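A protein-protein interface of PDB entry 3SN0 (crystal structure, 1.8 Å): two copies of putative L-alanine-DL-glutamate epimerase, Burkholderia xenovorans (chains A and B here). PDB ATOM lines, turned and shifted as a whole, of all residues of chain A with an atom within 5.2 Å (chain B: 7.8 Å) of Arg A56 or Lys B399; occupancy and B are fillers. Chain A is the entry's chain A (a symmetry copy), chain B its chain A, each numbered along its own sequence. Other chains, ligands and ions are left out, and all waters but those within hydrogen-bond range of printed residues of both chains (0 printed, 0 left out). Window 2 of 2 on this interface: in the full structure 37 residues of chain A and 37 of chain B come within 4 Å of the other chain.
Arg A56 touches one residue of chain B.
Lys B399 touches two residues of chain A.
Printed residues of chain A within 4 Å of Leu B395: Leu A75 (3.4 Å).
Of the printed residues of chain B, Gln A52 touches Leu B396 (3.9 Å).
Printed residues of chain B within 4 Å of Glu A71: Phe B185 (3.7 Å) and Lys B399 (3.4 Å).
Gly A54 touches none of the printed residues of chain B.
Glu B402 touches none of the printed residues of chain A.
The nearest residue of chain B that does not touch Arg A56 is Arg B400 (5.3 Å).
The nearest residue of chain A that does not touch Lys B399 is Leu A75 (4.4 Å).
No position is printed for both chains.
Of the 6 pairs that touch across the chains among the printed residues, none has its exchanged pair printed and touching as well.
Hydrophobic or aromatic side chains of chain B that line the printed part of chain A: Phe B185, Leu B395 and Leu B396.
Among the printed residues, 6 pairs touch across the chains.
Among the printed residues, no Asp or Glu carboxylate lies within 4 Å of a Lys or Arg side-chain nitrogen of the other chain.
Leu B396 touches Gln A52.
CE of Lys B399 touches NH2 of Arg A56, at 3.5 Å.
CE1 of Phe B185 touches N of Glu A71, at 3.7 Å.
Lys B399 touches Glu A71 (CE to OE2, 3.4 Å).
CD2 of Leu A75 touches O of Phe B181, 3.6 Å away.
Leu A75 touches Leu B395 (O to CD1, 3.4 Å).
The side-chain amino group (NZ) of Lys B399 lies within hydrogen-bond range of the backbone carbonyl oxygen (O) of Ala B182, 2.7 Å away.
NZ of Lys B399 lies within salt-bridge range of OE2 of Glu B402 (2.8 Å).
The guanidinium group (NH2) of Arg A56 lies within salt-bridge range of the side-chain carboxylate (OE2) of Glu A71 (2.5 Å).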
ATOM      1  N   GLN A  52      -0.019  37.061  17.529  1.00  0.00           N
ATOM      2  CA  GLN A  52       0.073  36.064  16.454  1.00  0.00           C
ATOM      3  C   GLN A  52      -0.881  34.904  16.699  1.00  0.00           C
ATOM      4  O   GLN A  52      -1.648  34.530  15.828  1.00  0.00           O
ATOM      5  CB  GLN A  52       1.500  35.520  16.300  1.00  0.00           C
ATOM      6  CG  GLN A  52       2.503  36.520  15.773  1.00  0.00           C
ATOM      7  CD  GLN A  52       2.151  37.052  14.393  1.00  0.00           C
ATOM      8  OE1 GLN A  52       1.421  36.419  13.634  1.00  0.00           O
ATOM      9  NE2 GLN A  52       2.678  38.225  14.064  1.00  0.00           N
ATOM     10  N   LEU A  53      -0.844  34.326  17.895  1.00  0.00           N
ATOM     11  CA  LEU A  53      -1.650  33.138  18.170  1.00  0.00           C
ATOM     12  C   LEU A  53      -3.145  33.415  18.199  1.00  0.00           C
ATOM     13  O   LEU A  53      -3.932  32.567  17.796  1.00  0.00           O
ATOM     14  CB  LEU A  53      -1.199  32.458  19.468  1.00  0.00           C
ATOM     15  CG  LEU A  53       0.188  31.824  19.413  1.00  0.00           C
ATOM     16  CD1 LEU A  53       0.547  31.204  20.776  1.00  0.00           C
ATOM     17  CD2 LEU A  53       0.260  30.739  18.318  1.00  0.00           C
ATOM     18  N   GLY A  54      -3.540  34.610  18.636  1.00  0.00           N
ATOM     19  CA  GLY A  54      -4.957  34.965  18.702  1.00  0.00           C
ATOM     20  C   GLY A  54      -5.609  35.056  17.330  1.00  0.00           C
ATOM     21  O   GLY A  54      -6.814  34.869  17.192  1.00  0.00           O
ATOM     22  N   LYS A  55      -4.810  35.331  16.304  1.00  0.00           N
ATOM     23  CA  LYS A  55      -5.329  35.355  14.939  1.00  0.00           C
ATOM     24  C   LYS A  55      -5.911  34.006  14.504  1.00  0.00           C
ATOM     25  O   LYS A  55      -6.869  33.977  13.748  1.00  0.00           O
ATOM     26  CB  LYS A  55      -4.250  35.805  13.954  1.00  0.00           C
ATOM     27  CG  LYS A  55      -3.813  37.248  14.182  1.00  0.00           C
ATOM     28  CD  LYS A  55      -2.766  37.706  13.192  1.00  0.00           C
ATOM     29  CE  LYS A  55      -2.108  39.004  13.673  1.00  0.00           C
ATOM     30  NZ  LYS A  55      -2.093  40.063  12.627  1.00  0.00           N
ATOM     31  N   ARG A  56      -5.321  32.904  14.961  1.00  0.00           N
ATOM     32  CA  ARG A  56      -5.796  31.566  14.601  1.00  0.00           C
ATOM     33  C   ARG A  56      -7.063  31.227  15.368  1.00  0.00           C
ATOM     34  O   ARG A  56      -7.865  30.392  14.944  1.00  0.00           O
ATOM     35  CB  ARG A  56      -4.746  30.507  14.949  1.00  0.00           C
ATOM     36  CG  ARG A  56      -3.473  30.517  14.093  1.00  0.00           C
ATOM     37  CD  ARG A  56      -3.554  29.566  12.878  1.00  0.00           C
ATOM     38  NE  ARG A  56      -4.413  28.395  13.105  1.00  0.00           N
ATOM     39  CZ  ARG A  56      -5.340  27.933  12.255  1.00  0.00           C
ATOM     40  NH1 ARG A  56      -5.542  28.498  11.057  1.00  0.00           N
ATOM     41  NH2 ARG A  56      -6.074  26.867  12.584  1.00  0.00           N
ATOM     42  N   LEU A  57      -7.224  31.855  16.522  1.00  0.00           N
ATOM     43  CA  LEU A  57      -8.359  31.571  17.392  1.00  0.00           C
ATOM     44  C   LEU A  57      -9.668  32.179  16.891  1.00  0.00           C
ATOM     45  O   LEU A  57     -10.744  31.624  17.121  1.00  0.00           O
ATOM     46  CB  LEU A  57      -8.033  32.056  18.818  1.00  0.00           C
ATOM     47  CG  LEU A  57      -9.006  31.698  19.932  1.00  0.00           C
ATOM     48  CD1 LEU A  57      -9.254  30.166  19.959  1.00  0.00           C
ATOM     49  CD2 LEU A  57      -8.481  32.238  21.289  1.00  0.00           C
ATOM     50  N   VAL A  58      -9.605  33.328  16.226  1.00  0.00           N
ATOM     51  CA  VAL A  58     -10.815  33.952  15.699  1.00  0.00           C
ATOM     52  C   VAL A  58     -11.521  33.003  14.718  1.00  0.00           C
ATOM     53  O   VAL A  58     -10.901  32.471  13.801  1.00  0.00           O
ATOM     54  CB  VAL A  58     -10.511  35.296  15.021  1.00  0.00           C
ATOM     55  CG1 VAL A  58     -11.737  35.836  14.311  1.00  0.00           C
ATOM     56  CG2 VAL A  58      -9.992  36.321  16.075  1.00  0.00           C
ATOM     57  N   ALA A  60     -12.889  30.168  15.749  1.00  0.00           N
ATOM     58  CA  ALA A  60     -12.959  28.895  16.480  1.00  0.00           C
ATOM     59  C   ALA A  60     -13.926  28.974  17.655  1.00  0.00           C
ATOM     60  O   ALA A  60     -14.339  30.055  18.066  1.00  0.00           O
ATOM     61  CB  ALA A  60     -11.578  28.476  16.970  1.00  0.00           C
ATOM     62  N   GLU A  71      -3.367  22.926  19.356  1.00  0.00           N
ATOM     63  CA  GLU A  71      -2.967  23.534  18.095  1.00  0.00           C
ATOM     64  C   GLU A  71      -1.805  24.519  18.301  1.00  0.00           C
ATOM     65  O   GLU A  71      -0.823  24.520  17.551  1.00  0.00           O
ATOM     66  CB  GLU A  71      -4.129  24.282  17.472  1.00  0.00           C
ATOM     67  CG  GLU A  71      -3.814  24.803  16.091  1.00  0.00           C
ATOM     68  CD  GLU A  71      -4.977  25.532  15.465  1.00  0.00           C
ATOM     69  OE1 GLU A  71      -5.519  26.440  16.079  1.00  0.00           O
ATOM     70  OE2 GLU A  71      -5.342  25.205  14.338  1.00  0.00           O
ATOM     71  N   LEU A  75       1.972  24.605  16.700  1.00  0.00           N
ATOM     72  CA  LEU A  75       2.448  25.704  15.872  1.00  0.00           C
ATOM     73  C   LEU A  75       3.700  26.409  16.428  1.00  0.00           C
ATOM     74  O   LEU A  75       4.364  27.137  15.689  1.00  0.00           O
ATOM     75  CB  LEU A  75       1.347  26.728  15.665  1.00  0.00           C
ATOM     76  CG  LEU A  75       0.140  26.247  14.859  1.00  0.00           C
ATOM     77  CD1 LEU A  75      -0.953  27.326  14.850  1.00  0.00           C
ATOM     78  CD2 LEU A  75       0.556  25.884  13.437  1.00  0.00           C
ATOM     79  N   ARG B 178       2.691  16.554   8.339  1.00  0.00           N
ATOM     80  CA  ARG B 178       3.309  17.389   9.365  1.00  0.00           C
ATOM     81  C   ARG B 178       2.403  17.580  10.595  1.00  0.00           C
ATOM     82  O   ARG B 178       2.226  18.710  11.059  1.00  0.00           O
ATOM     83  CB  ARG B 178       3.652  18.769   8.763  1.00  0.00           C
ATOM     84  CG  ARG B 178       4.610  18.703   7.546  1.00  0.00           C
ATOM     85  CD  ARG B 178       4.638  20.028   6.774  1.00  0.00           C
ATOM     86  NE  ARG B 178       5.144  21.090   7.625  1.00  0.00           N
ATOM     87  CZ  ARG B 178       4.404  22.024   8.215  1.00  0.00           C
ATOM     88  NH1 ARG B 178       5.000  22.904   9.005  1.00  0.00           N
ATOM     89  NH2 ARG B 178       3.075  22.100   8.024  1.00  0.00           N
ATOM     90  N   PHE B 181       3.274  19.792  13.592  1.00  0.00           N
ATOM     91  CA  PHE B 181       3.096  21.225  13.371  1.00  0.00           C
ATOM     92  C   PHE B 181       1.677  21.561  12.926  1.00  0.00           C
ATOM     93  O   PHE B 181       1.430  22.621  12.319  1.00  0.00           O
ATOM     94  CB  PHE B 181       4.126  21.716  12.341  1.00  0.00           C
ATOM     95  CG  PHE B 181       5.578  21.529  12.756  1.00  0.00           C
ATOM     96  CD1 PHE B 181       5.999  21.691  14.083  1.00  0.00           C
ATOM     97  CD2 PHE B 181       6.556  21.220  11.788  1.00  0.00           C
ATOM     98  CE1 PHE B 181       7.341  21.534  14.428  1.00  0.00           C
ATOM     99  CE2 PHE B 181       7.875  21.053  12.129  1.00  0.00           C
ATOM    100  CZ  PHE B 181       8.283  21.215  13.463  1.00  0.00           C
ATOM    101  N   ALA B 182       0.742  20.671  13.261  1.00  0.00           N
ATOM    102  CA  ALA B 182      -0.689  20.883  13.059  1.00  0.00           C
ATOM    103  C   ALA B 182      -1.191  20.858  11.603  1.00  0.00           C
ATOM    104  O   ALA B 182      -2.307  21.329  11.339  1.00  0.00           O
ATOM    105  CB  ALA B 182      -1.131  22.174  13.750  1.00  0.00           C
ATOM    106  N   VAL B 183      -0.419  20.303  10.667  1.00  0.00           N
ATOM    107  CA  VAL B 183      -0.940  20.019   9.327  1.00  0.00           C
ATOM    108  C   VAL B 183      -0.698  18.559   8.931  1.00  0.00           C
ATOM    109  O   VAL B 183       0.397  18.204   8.513  1.00  0.00           O
ATOM    110  CB  VAL B 183      -0.343  20.933   8.243  1.00  0.00           C
ATOM    111  CG1 VAL B 183      -1.046  20.684   6.901  1.00  0.00           C
ATOM    112  CG2 VAL B 183      -0.449  22.401   8.671  1.00  0.00           C
ATOM    113  N   PRO B 184      -1.723  17.720   9.052  1.00  0.00           N
ATOM    114  CA  PRO B 184      -3.063  18.044   9.539  1.00  0.00           C
ATOM    115  C   PRO B 184      -3.129  18.161  11.062  1.00  0.00           C
ATOM    116  O   PRO B 184      -2.174  17.779  11.761  1.00  0.00           O
ATOM    117  CB  PRO B 184      -3.866  16.837   9.099  1.00  0.00           C
ATOM    118  CG  PRO B 184      -2.917  15.716   9.237  1.00  0.00           C
ATOM    119  CD  PRO B 184      -1.587  16.268   8.799  1.00  0.00           C
ATOM    120  N   PHE B 185      -4.272  18.633  11.570  1.00  0.00           N
ATOM    121  CA  PHE B 185      -4.451  18.709  13.006  1.00  0.00           C
ATOM    122  C   PHE B 185      -4.880  17.328  13.476  1.00  0.00           C
ATOM    123  O   PHE B 185      -6.055  16.923  13.341  1.00  0.00           O
ATOM    124  CB  PHE B 185      -5.448  19.790  13.418  1.00  0.00           C
ATOM    125  CG  PHE B 185      -5.652  19.880  14.908  1.00  0.00           C
ATOM    126  CD1 PHE B 185      -4.673  20.408  15.725  1.00  0.00           C
ATOM    127  CD2 PHE B 185      -6.811  19.401  15.492  1.00  0.00           C
ATOM    128  CE1 PHE B 185      -4.858  20.470  17.103  1.00  0.00           C
ATOM    129  CE2 PHE B 185      -6.990  19.470  16.853  1.00  0.00           C
ATOM    130  CZ  PHE B 185      -6.020  20.022  17.651  1.00  0.00           C
ATOM    131  N   GLN B 186      -3.902  16.593  13.986  1.00  0.00           N
ATOM    132  CA  GLN B 186      -4.109  15.252  14.521  1.00  0.00           C
ATOM    133  C   GLN B 186      -3.144  15.132  15.684  1.00  0.00           C
ATOM    134  O   GLN B 186      -2.053  14.573  15.538  1.00  0.00           O
ATOM    135  CB  GLN B 186      -3.785  14.197  13.464  1.00  0.00           C
ATOM    136  CG  GLN B 186      -4.747  14.179  12.311  1.00  0.00           C
ATOM    137  CD  GLN B 186      -4.547  13.000  11.384  1.00  0.00           C
ATOM    138  OE1 GLN B 186      -3.862  12.022  11.724  1.00  0.00           O
ATOM    139  NE2 GLN B 186      -5.148  13.081  10.202  1.00  0.00           N
ATOM    140  N   GLY B 393       4.994  34.061   8.381  1.00  0.00           N
ATOM    141  CA  GLY B 393       4.715  32.806   7.693  1.00  0.00           C
ATOM    142  C   GLY B 393       5.314  31.631   8.456  1.00  0.00           C
ATOM    143  O   GLY B 393       5.032  31.445   9.644  1.00  0.00           O
ATOM    144  N   GLY B 394       6.156  30.850   7.794  1.00  0.00           N
ATOM    145  CA  GLY B 394       6.786  29.703   8.448  1.00  0.00           C
ATOM    146  C   GLY B 394       5.715  28.715   8.871  1.00  0.00           C
ATOM    147  O   GLY B 394       4.817  28.404   8.081  1.00  0.00           O
ATOM    148  N   LEU B 395       5.772  28.245  10.116  1.00  0.00           N
ATOM    149  CA  LEU B 395       4.774  27.268  10.583  1.00  0.00           C
ATOM    150  C   LEU B 395       3.336  27.793  10.498  1.00  0.00           C
ATOM    151  O   LEU B 395       2.383  27.002  10.326  1.00  0.00           O
ATOM    152  CB  LEU B 395       5.083  26.767  12.000  1.00  0.00           C
ATOM    153  CG  LEU B 395       6.453  26.104  12.169  1.00  0.00           C
ATOM    154  CD1 LEU B 395       6.658  25.616  13.624  1.00  0.00           C
ATOM    155  CD2 LEU B 395       6.682  24.949  11.168  1.00  0.00           C
ATOM    156  N   LEU B 396       3.167  29.109  10.591  1.00  0.00           N
ATOM    157  CA  LEU B 396       1.820  29.705  10.478  1.00  0.00           C
ATOM    158  C   LEU B 396       1.226  29.726   9.062  1.00  0.00           C
ATOM    159  O   LEU B 396      -0.006  29.718   8.910  1.00  0.00           O
ATOM    160  CB  LEU B 396       1.808  31.114  11.044  1.00  0.00           C
ATOM    161  CG  LEU B 396       2.354  31.262  12.466  1.00  0.00           C
ATOM    162  CD1 LEU B 396       1.923  32.616  12.991  1.00  0.00           C
ATOM    163  CD2 LEU B 396       1.864  30.151  13.405  1.00  0.00           C
ATOM    164  N   GLN B 397       2.061  29.745   8.027  1.00  0.00           N
ATOM    165  CA  GLN B 397       1.529  29.835   6.655  1.00  0.00           C
ATOM    166  C   GLN B 397       1.207  28.487   5.993  1.00  0.00           C
ATOM    167  O   GLN B 397       0.424  28.453   5.033  1.00  0.00           O
ATOM    168  CB  GLN B 397       2.439  30.675   5.755  1.00  0.00           C
ATOM    169  CG  GLN B 397       3.630  29.959   5.175  1.00  0.00           C
ATOM    170  CD  GLN B 397       3.360  29.344   3.814  1.00  0.00           C
ATOM    171  OE1 GLN B 397       2.905  30.023   2.890  1.00  0.00           O
ATOM    172  NE2 GLN B 397       3.661  28.053   3.676  1.00  0.00           N
ATOM    173  N   TYR B 398       1.809  27.392   6.470  1.00  0.00           N
ATOM    174  CA  TYR B 398       1.368  26.048   6.049  1.00  0.00           C
ATOM    175  C   TYR B 398      -0.096  25.871   6.442  1.00  0.00           C
ATOM    176  O   TYR B 398      -0.888  25.281   5.709  1.00  0.00           O
ATOM    177  CB  TYR B 398       2.161  24.933   6.740  1.00  0.00           C
ATOM    178  CG  TYR B 398       3.618  24.803   6.350  1.00  0.00           C
ATOM    179  CD1 TYR B 398       4.009  23.999   5.279  1.00  0.00           C
ATOM    180  CD2 TYR B 398       4.608  25.449   7.081  1.00  0.00           C
ATOM    181  CE1 TYR B 398       5.355  23.861   4.934  1.00  0.00           C
ATOM    182  CE2 TYR B 398       5.945  25.324   6.745  1.00  0.00           C
ATOM    183  CZ  TYR B 398       6.315  24.531   5.670  1.00  0.00           C
ATOM    184  OH  TYR B 398       7.634  24.410   5.350  1.00  0.00           O
ATOM    185  N   LYS B 399      -0.422  26.372   7.632  1.00  0.00           N
ATOM    186  CA  LYS B 399      -1.760  26.258   8.196  1.00  0.00           C
ATOM    187  C   LYS B 399      -2.769  27.156   7.437  1.00  0.00           C
ATOM    188  O   LYS B 399      -3.948  26.805   7.323  1.00  0.00           O
ATOM    189  CB  LYS B 399      -1.709  26.570   9.703  1.00  0.00           C
ATOM    190  CG  LYS B 399      -2.922  26.112  10.498  1.00  0.00           C
ATOM    191  CD  LYS B 399      -3.005  24.594  10.615  1.00  0.00           C
ATOM    192  CE  LYS B 399      -4.319  24.177  11.269  1.00  0.00           C
ATOM    193  NZ  LYS B 399      -4.573  22.721  11.168  1.00  0.00           N
ATOM    194  N   ARG B 400      -2.301  28.284   6.891  1.00  0.00           N
ATOM    195  CA  ARG B 400      -3.116  29.093   5.962  1.00  0.00           C
ATOM    196  C   ARG B 400      -3.366  28.351   4.649  1.00  0.00           C
ATOM    197  O   ARG B 400      -4.504  28.273   4.178  1.00  0.00           O
ATOM    198  CB  ARG B 400      -2.446  30.436   5.646  1.00  0.00           C
ATOM    199  CG  ARG B 400      -2.512  31.437   6.772  1.00  0.00           C
ATOM    200  CD  ARG B 400      -2.243  32.868   6.282  1.00  0.00           C
ATOM    201  NE  ARG B 400      -1.956  33.736   7.423  1.00  0.00           N
ATOM    202  CZ  ARG B 400      -0.742  33.986   7.918  1.00  0.00           C
ATOM    203  NH1 ARG B 400       0.361  33.465   7.362  1.00  0.00           N
ATOM    204  NH2 ARG B 400      -0.622  34.783   8.979  1.00  0.00           N
ATOM    205  N   SER B 401      -2.289  27.821   4.064  1.00  0.00           N
ATOM    206  CA  SER B 401      -2.368  27.033   2.826  1.00  0.00           C
ATOM    207  C   SER B 401      -3.377  25.892   2.963  1.00  0.00           C
ATOM    208  O   SER B 401      -4.098  25.574   2.015  1.00  0.00           O
ATOM    209  CB  SER B 401      -0.995  26.453   2.454  1.00  0.00           C
ATOM    210  OG  SER B 401      -0.011  27.466   2.349  1.00  0.00           O
ATOM    211  N   GLU B 402      -3.415  25.282   4.146  1.00  0.00           N
ATOM    212  CA  GLU B 402      -4.377  24.221   4.441  1.00  0.00           C
ATOM    213  C   GLU B 402      -5.808  24.775   4.421  1.00  0.00           C
ATOM    214  O   GLU B 402      -6.684  24.220   3.758  1.00  0.00           O
ATOM    215  CB  GLU B 402      -4.080  23.584   5.808  1.00  0.00           C
ATOM    216  CG  GLU B 402      -4.754  22.233   6.013  1.00  0.00           C
ATOM    217  CD  GLU B 402      -4.807  21.793   7.473  1.00  0.00           C
ATOM    218  OE1 GLU B 402      -4.798  20.566   7.714  1.00  0.00           O
ATOM    219  OE2 GLU B 402      -4.869  22.664   8.372  1.00  0.00           O
